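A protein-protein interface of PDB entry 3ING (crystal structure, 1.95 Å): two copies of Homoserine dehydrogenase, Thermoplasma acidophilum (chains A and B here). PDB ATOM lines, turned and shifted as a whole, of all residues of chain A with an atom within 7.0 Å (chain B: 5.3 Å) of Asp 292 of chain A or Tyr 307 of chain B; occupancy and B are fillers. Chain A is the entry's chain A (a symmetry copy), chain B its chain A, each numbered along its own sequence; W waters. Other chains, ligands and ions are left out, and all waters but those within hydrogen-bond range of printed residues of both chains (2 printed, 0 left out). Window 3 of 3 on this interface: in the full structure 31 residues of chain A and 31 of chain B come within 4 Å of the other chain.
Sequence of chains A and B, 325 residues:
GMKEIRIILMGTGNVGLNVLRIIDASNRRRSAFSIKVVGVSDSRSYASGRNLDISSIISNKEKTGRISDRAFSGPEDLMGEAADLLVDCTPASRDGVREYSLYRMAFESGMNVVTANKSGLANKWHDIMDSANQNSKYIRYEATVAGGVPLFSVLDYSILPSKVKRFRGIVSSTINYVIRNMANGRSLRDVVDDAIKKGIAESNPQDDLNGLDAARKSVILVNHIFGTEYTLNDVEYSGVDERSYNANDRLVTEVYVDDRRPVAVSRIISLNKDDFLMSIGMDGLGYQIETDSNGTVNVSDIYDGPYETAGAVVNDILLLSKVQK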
ATOM      1  N   PRO A 161       6.820 -16.338 -32.085  1.00  0.00           N
ATOM      2  CA  PRO A 161       6.829 -15.738 -30.761  1.00  0.00           C
ATOM      3  C   PRO A 161       7.790 -16.353 -29.738  1.00  0.00           C
ATOM      4  O   PRO A 161       8.015 -15.761 -28.689  1.00  0.00           O
ATOM      5  CB  PRO A 161       5.408 -15.982 -30.257  1.00  0.00           C
ATOM      6  CG  PRO A 161       4.668 -16.526 -31.370  1.00  0.00           C
ATOM      7  CD  PRO A 161       5.590 -17.085 -32.341  1.00  0.00           C
ATOM      8  N   SER A 162       8.338 -17.521 -30.028  1.00  0.00           N
ATOM      9  CA  SER A 162       9.065 -18.285 -29.017  1.00  0.00           C
ATOM     10  C   SER A 162      10.569 -18.162 -28.996  1.00  0.00           C
ATOM     11  O   SER A 162      11.221 -17.997 -30.044  1.00  0.00           O
ATOM     12  CB  SER A 162       8.833 -19.779 -29.265  1.00  0.00           C
ATOM     13  OG  SER A 162       7.545 -20.202 -28.838  1.00  0.00           O
ATOM     14  N   LYS A 163      11.112 -18.350 -27.803  1.00  0.00           N
ATOM     15  CA  LYS A 163      12.493 -18.792 -27.682  1.00  0.00           C
ATOM     16  C   LYS A 163      12.487 -20.345 -27.714  1.00  0.00           C
ATOM     17  O   LYS A 163      11.653 -20.980 -27.090  1.00  0.00           O
ATOM     18  CB  LYS A 163      13.094 -18.319 -26.380  1.00  0.00           C
ATOM     19  CG  LYS A 163      13.291 -16.818 -26.299  1.00  0.00           C
ATOM     20  CD  LYS A 163      13.904 -16.392 -24.955  1.00  0.00           C
ATOM     21  CE  LYS A 163      14.324 -14.911 -24.964  1.00  0.00           C
ATOM     22  NZ  LYS A 163      14.647 -14.339 -23.595  1.00  0.00           N
ATOM     23  N   VAL A 164      13.396 -20.931 -28.472  1.00  0.00           N
ATOM     24  CA  VAL A 164      13.604 -22.374 -28.505  1.00  0.00           C
ATOM     25  C   VAL A 164      14.571 -22.713 -27.404  1.00  0.00           C
ATOM     26  O   VAL A 164      15.698 -22.156 -27.325  1.00  0.00           O
ATOM     27  CB  VAL A 164      14.200 -22.896 -29.829  1.00  0.00           C
ATOM     28  CG1 VAL A 164      14.536 -24.384 -29.705  1.00  0.00           C
ATOM     29  CG2 VAL A 164      13.238 -22.668 -30.980  1.00  0.00           C
ATOM     30  N   LYS A 165      14.131 -23.587 -26.526  1.00  0.00           N
ATOM     31  CA  LYS A 165      14.948 -24.015 -25.378  1.00  0.00           C
ATOM     32  C   LYS A 165      15.791 -25.231 -25.755  1.00  0.00           C
ATOM     33  O   LYS A 165      16.953 -25.339 -25.368  1.00  0.00           O
ATOM     34  CB  LYS A 165      14.071 -24.363 -24.192  1.00  0.00           C
ATOM     35  CG  LYS A 165      12.945 -23.320 -23.818  1.00  0.00           C
ATOM     36  CD  LYS A 165      13.420 -21.908 -23.391  1.00  0.00           C
ATOM     37  N   GLU A 290      11.338 -27.923 -28.064  1.00  0.00           N
ATOM     38  CA  GLU A 290      10.753 -27.313 -26.865  1.00  0.00           C
ATOM     39  C   GLU A 290      10.852 -25.804 -26.970  1.00  0.00           C
ATOM     40  O   GLU A 290      11.939 -25.296 -27.160  1.00  0.00           O
ATOM     41  CB  GLU A 290      11.479 -27.747 -25.594  1.00  0.00           C
ATOM     42  CG  GLU A 290      11.583 -29.221 -25.396  1.00  0.00           C
ATOM     43  CD  GLU A 290      12.320 -29.605 -24.108  1.00  0.00           C
ATOM     44  OE1 GLU A 290      12.759 -28.699 -23.352  1.00  0.00           O
ATOM     45  OE2 GLU A 290      12.450 -30.822 -23.856  1.00  0.00           O
ATOM     46  N   THR A 291       9.718 -25.108 -26.822  1.00  0.00           N
ATOM     47  CA  THR A 291       9.613 -23.646 -26.965  1.00  0.00           C
ATOM     48  C   THR A 291       8.961 -23.029 -25.775  1.00  0.00           C
ATOM     49  O   THR A 291       8.218 -23.692 -25.048  1.00  0.00           O
ATOM     50  CB  THR A 291       8.797 -23.199 -28.214  1.00  0.00           C
ATOM     51  OG1 THR A 291       7.368 -23.321 -27.999  1.00  0.00           O
ATOM     52  CG2 THR A 291       9.216 -23.970 -29.451  1.00  0.00           C
ATOM     53  N   ASP A 292       9.172 -21.727 -25.592  1.00  0.00           N
ATOM     54  CA  ASP A 292       8.594 -21.102 -24.442  1.00  0.00           C
ATOM     55  C   ASP A 292       7.193 -20.501 -24.701  1.00  0.00           C
ATOM     56  O   ASP A 292       6.526 -20.165 -23.747  1.00  0.00           O
ATOM     57  CB  ASP A 292       9.567 -20.098 -23.815  1.00  0.00           C
ATOM     58  CG  ASP A 292       9.761 -18.836 -24.657  1.00  0.00           C
ATOM     59  OD1 ASP A 292       9.217 -18.777 -25.757  1.00  0.00           O
ATOM     60  OD2 ASP A 292      10.478 -17.907 -24.214  1.00  0.00           O
ATOM     61  N   SER A 293       6.777 -20.363 -25.976  1.00  0.00           N
ATOM     62  CA  SER A 293       5.445 -19.797 -26.306  1.00  0.00           C
ATOM     63  C   SER A 293       4.559 -20.608 -27.272  1.00  0.00           C
ATOM     64  O   SER A 293       3.397 -20.239 -27.528  1.00  0.00           O
ATOM     65  CB  SER A 293       5.638 -18.406 -26.898  1.00  0.00           C
ATOM     66  OG  SER A 293       6.402 -17.591 -26.033  1.00  0.00           O
ATOM     67  N   ASN A 294       5.080 -21.699 -27.797  1.00  0.00           N
ATOM     68  CA  ASN A 294       4.340 -22.551 -28.741  1.00  0.00           C
ATOM     69  C   ASN A 294       4.373 -24.018 -28.344  1.00  0.00           C
ATOM     70  O   ASN A 294       4.149 -24.904 -29.190  1.00  0.00           O
ATOM     71  CB  ASN A 294       4.918 -22.363 -30.165  1.00  0.00           C
ATOM     72  CG  ASN A 294       4.684 -20.962 -30.698  1.00  0.00           C
ATOM     73  OD1 ASN A 294       3.601 -20.684 -31.256  1.00  0.00           O
ATOM     74  ND2 ASN A 294       5.671 -20.051 -30.503  1.00  0.00           N
ATOM     75  N   GLY A 295       4.640 -24.275 -27.058  1.00  0.00           N
ATOM     76  CA  GLY A 295       4.700 -25.636 -26.539  1.00  0.00           C
ATOM     77  C   GLY A 295       5.881 -26.446 -27.028  1.00  0.00           C
ATOM     78  O   GLY A 295       6.936 -25.884 -27.379  1.00  0.00           O
ATOM     79  N   ASN B  14      -9.724 -17.835 -21.781  1.00  0.00           N
ATOM     80  CA  ASN B  14      -8.594 -18.765 -21.716  1.00  0.00           C
ATOM     81  C   ASN B  14      -7.538 -18.430 -22.749  1.00  0.00           C
ATOM     82  O   ASN B  14      -6.343 -18.375 -22.459  1.00  0.00           O
ATOM     83  CB  ASN B  14      -9.067 -20.203 -21.947  1.00  0.00           C
ATOM     84  CG  ASN B  14      -9.897 -20.728 -20.810  1.00  0.00           C
ATOM     85  OD1 ASN B  14     -10.066 -20.048 -19.826  1.00  0.00           O
ATOM     86  ND2 ASN B  14     -10.459 -21.911 -20.957  1.00  0.00           N
ATOM     87  N   ASN B  18      -4.169 -15.210 -22.457  1.00  0.00           N
ATOM     88  CA  ASN B  18      -2.833 -15.729 -22.779  1.00  0.00           C
ATOM     89  C   ASN B  18      -2.212 -15.022 -23.972  1.00  0.00           C
ATOM     90  O   ASN B  18      -0.991 -14.938 -24.099  1.00  0.00           O
ATOM     91  CB  ASN B  18      -2.876 -17.253 -23.021  1.00  0.00           C
ATOM     92  CG  ASN B  18      -2.842 -18.049 -21.727  1.00  0.00           C
ATOM     93  OD1 ASN B  18      -2.067 -17.727 -20.844  1.00  0.00           O
ATOM     94  ND2 ASN B  18      -3.699 -19.069 -21.611  1.00  0.00           N
ATOM     95  N   ILE B  22       1.467 -13.396 -23.705  1.00  0.00           N
ATOM     96  CA  ILE B  22       2.539 -13.645 -24.680  1.00  0.00           C
ATOM     97  C   ILE B  22       3.027 -12.356 -25.304  1.00  0.00           C
ATOM     98  O   ILE B  22       4.226 -12.138 -25.404  1.00  0.00           O
ATOM     99  CB  ILE B  22       2.110 -14.685 -25.750  1.00  0.00           C
ATOM    100  CG1 ILE B  22       1.965 -16.052 -25.063  1.00  0.00           C
ATOM    101  CG2 ILE B  22       3.146 -14.793 -26.906  1.00  0.00           C
ATOM    102  CD1 ILE B  22       1.393 -17.173 -25.901  1.00  0.00           C
ATOM    103  N   ARG B  29      11.151  -8.534 -24.230  1.00  0.00           N
ATOM    104  CA  ARG B  29      12.407  -9.014 -24.799  1.00  0.00           C
ATOM    105  C   ARG B  29      12.953  -7.989 -25.755  1.00  0.00           C
ATOM    106  O   ARG B  29      14.154  -7.735 -25.772  1.00  0.00           O
ATOM    107  CB  ARG B  29      12.190 -10.292 -25.588  1.00  0.00           C
ATOM    108  CG  ARG B  29      11.868 -11.492 -24.754  1.00  0.00           C
ATOM    109  CD  ARG B  29      11.217 -12.548 -25.618  1.00  0.00           C
ATOM    110  NE  ARG B  29      11.987 -12.851 -26.830  1.00  0.00           N
ATOM    111  CZ  ARG B  29      11.552 -13.622 -27.830  1.00  0.00           C
ATOM    112  NH1 ARG B  29      10.346 -14.180 -27.786  1.00  0.00           N
ATOM    113  NH2 ARG B  29      12.328 -13.839 -28.887  1.00  0.00           N
ATOM    114  N   GLY B 305      -2.919 -26.631 -25.144  1.00  0.00           N
ATOM    115  CA  GLY B 305      -3.800 -25.899 -24.253  1.00  0.00           C
ATOM    116  C   GLY B 305      -4.015 -24.512 -24.771  1.00  0.00           C
ATOM    117  O   GLY B 305      -3.496 -24.170 -25.838  1.00  0.00           O
ATOM    118  N   PRO B 306      -4.782 -23.699 -24.025  1.00  0.00           N
ATOM    119  CA  PRO B 306      -5.045 -22.318 -24.438  1.00  0.00           C
ATOM    120  C   PRO B 306      -3.793 -21.440 -24.501  1.00  0.00           C
ATOM    121  O   PRO B 306      -3.769 -20.485 -25.263  1.00  0.00           O
ATOM    122  CB  PRO B 306      -6.036 -21.821 -23.382  1.00  0.00           C
ATOM    123  CG  PRO B 306      -5.832 -22.717 -22.230  1.00  0.00           C
ATOM    124  CD  PRO B 306      -5.464 -24.034 -22.779  1.00  0.00           C
ATOM    125  N   TYR B 307      -2.751 -21.772 -23.749  1.00  0.00           N
ATOM    126  CA  TYR B 307      -1.511 -20.999 -23.838  1.00  0.00           C
ATOM    127  C   TYR B 307      -0.837 -21.200 -25.218  1.00  0.00           C
ATOM    128  O   TYR B 307      -0.358 -20.271 -25.830  1.00  0.00           O
ATOM    129  CB  TYR B 307      -0.572 -21.364 -22.706  1.00  0.00           C
ATOM    130  CG  TYR B 307       0.741 -20.637 -22.771  1.00  0.00           C
ATOM    131  CD1 TYR B 307       0.845 -19.310 -22.384  1.00  0.00           C
ATOM    132  CD2 TYR B 307       1.876 -21.279 -23.242  1.00  0.00           C
ATOM    133  CE1 TYR B 307       2.037 -18.635 -22.471  1.00  0.00           C
ATOM    134  CE2 TYR B 307       3.081 -20.623 -23.306  1.00  0.00           C
ATOM    135  CZ  TYR B 307       3.148 -19.298 -22.933  1.00  0.00           C
ATOM    136  OH  TYR B 307       4.349 -18.656 -23.041  1.00  0.00           O
ATOM    137  N   GLU B 308      -0.757 -22.459 -25.646  1.00  0.00           N
ATOM    138  CA  GLU B 308      -0.191 -22.847 -26.939  1.00  0.00           C
ATOM    139  C   GLU B 308      -1.029 -22.351 -28.079  1.00  0.00           C
ATOM    140  O   GLU B 308      -0.511 -21.917 -29.101  1.00  0.00           O
ATOM    141  CB  GLU B 308      -0.026 -24.364 -26.999  1.00  0.00           C
ATOM    142  CG  GLU B 308       0.994 -24.882 -25.970  1.00  0.00           C
ATOM    143  CD  GLU B 308       0.485 -25.037 -24.540  1.00  0.00           C
ATOM    144  OE1 GLU B 308      -0.734 -25.063 -24.278  1.00  0.00           O
ATOM    145  OE2 GLU B 308       1.337 -25.230 -23.670  1.00  0.00           O
ATOM    146  N   THR B 309      -2.334 -22.359 -27.903  1.00  0.00           N
ATOM    147  CA  THR B 309      -3.229 -21.789 -28.890  1.00  0.00           C
ATOM    148  C   THR B 309      -2.950 -20.293 -29.009  1.00  0.00           C
ATOM    149  O   THR B 309      -2.869 -19.759 -30.108  1.00  0.00           O
ATOM    150  CB  THR B 309      -4.696 -22.029 -28.456  1.00  0.00           C
ATOM    151  OG1 THR B 309      -4.963 -23.445 -28.378  1.00  0.00           O
ATOM    152  CG2 THR B 309      -5.748 -21.361 -29.399  1.00  0.00           C
ATOM    153  N   ALA B 310      -2.792 -19.611 -27.880  1.00  0.00           N
ATOM    154  CA  ALA B 310      -2.429 -18.170 -27.876  1.00  0.00           C
ATOM    155  C   ALA B 310      -1.103 -17.907 -28.642  1.00  0.00           C
ATOM    156  O   ALA B 310      -0.928 -16.911 -29.339  1.00  0.00           O
ATOM    157  CB  ALA B 310      -2.356 -17.649 -26.393  1.00  0.00           C
ATOM    158  N   GLY B 311      -0.174 -18.840 -28.545  1.00  0.00           N
ATOM    159  CA  GLY B 311       1.087 -18.703 -29.242  1.00  0.00           C
ATOM    160  C   GLY B 311       0.888 -18.791 -30.745  1.00  0.00           C
ATOM    161  O   GLY B 311       1.533 -18.086 -31.483  1.00  0.00           O
HETATM  162  O   HOH W   1       9.785 -15.239 -25.124  1.00  0.00           O
HETATM  163  O   HOH W   2       1.557 -22.665 -30.940  1.00  0.00           O
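Among the printed residues, pairs that only touch across the chains: Pro 161 of chain A with Gly 311 of chain B (3.5 Å), Lys 163 of chain A with Arg 29 of chain B (3.6 Å), Ser 293 of chain A with Tyr 307 of chain B (3.6 Å), Ser 293 of chain A with Gly 311 of chain B (3.3 Å) and Gly 295 of chain A with Glu 308 of chain B (3.8 Å).
No position is printed for both chains.
Printed residues of chain B that touch a printed residue of chain A: Arg 29, Tyr 307, Glu 308 and Gly 311. Hydrophobic or aromatic side chains of chain B that line the printed part of chain A: Tyr 307. Of the 11 printed residues of chain A, 6 touch a printed residue of chain B. Hydrophobic or aromatic side chains of chain A within 4 Å of the printed part of chain B: Pro 161.
N of Gly 305 of chain B sits at hydrogen-bond distance from OE1 of Glu 308 of chain B (2.8 Å). OG of Ser 162 of chain A is in hydrogen-bond range of ND2 of Asn 294 of chain A (2.5 Å). The backbone NH of Asn 294 of chain A lies within hydrogen-bond range of the side-chain hydroxyl of Thr 291 of chain A (2.8 Å). The backbone NH (N) of Lys 163 of chain A is in hydrogen-bond range of the side-chain carboxylate (OD1) of Asp 292 of chain A (2.8 Å). The backbone carbonyl oxygen (O) of Gly 295 of chain A lies within hydrogen-bond range of the side-chain hydroxyl (OG1) of Thr 291 of chain A (2.7 Å). The side-chain hydroxyl (OG) of Ser 162 of chain A is in hydrogen-bond range of the backbone NH (N) of Ser 293 of chain A (3.0 Å).
Of chain B, only Tyr 307 (2.7 Å) comes within 4 Å of Asp 292 of chain A. Of the printed residues of chain A, Gly 311 of chain B touches Pro 161 (3.5 Å), Ser 293 (3.3 Å) and Asn 294 (3.3 Å). Of the printed residues of chain A, Glu 308 of chain B touches Gly 295 (3.8 Å). Asn 18 of chain B touches none of the printed residues of chain A. The nearest printed residue of chain B that does not touch Asn 294 of chain A is Glu 308 of chain B (4.2 Å).
The side-chain hydroxyl (OH) of Tyr 307 of chain B lies within hydrogen-bond range of the backbone carbonyl oxygen (O) of Asp 292 of chain A, 2.7 Å away. The guanidinium group of Arg 29 of chain B lies within hydrogen-bond range of the backbone carbonyl oxygen of Pro 161 of chain A (3.0 Å). OD1 of Asn 294 of chain A sits close to O of Gly 311 of chain B (3.3 Å).
Water W2 lies within hydrogen-bond range of OD1 of Asn 294 of chain A (2.9 Å) and O of Glu 308 of chain B (2.9 Å). Water W1 lies within hydrogen-bond range of OD2 of Asp 292 of chain A (2.9 Å) and NH1 of Arg 29 of chain B (2.9 Å).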
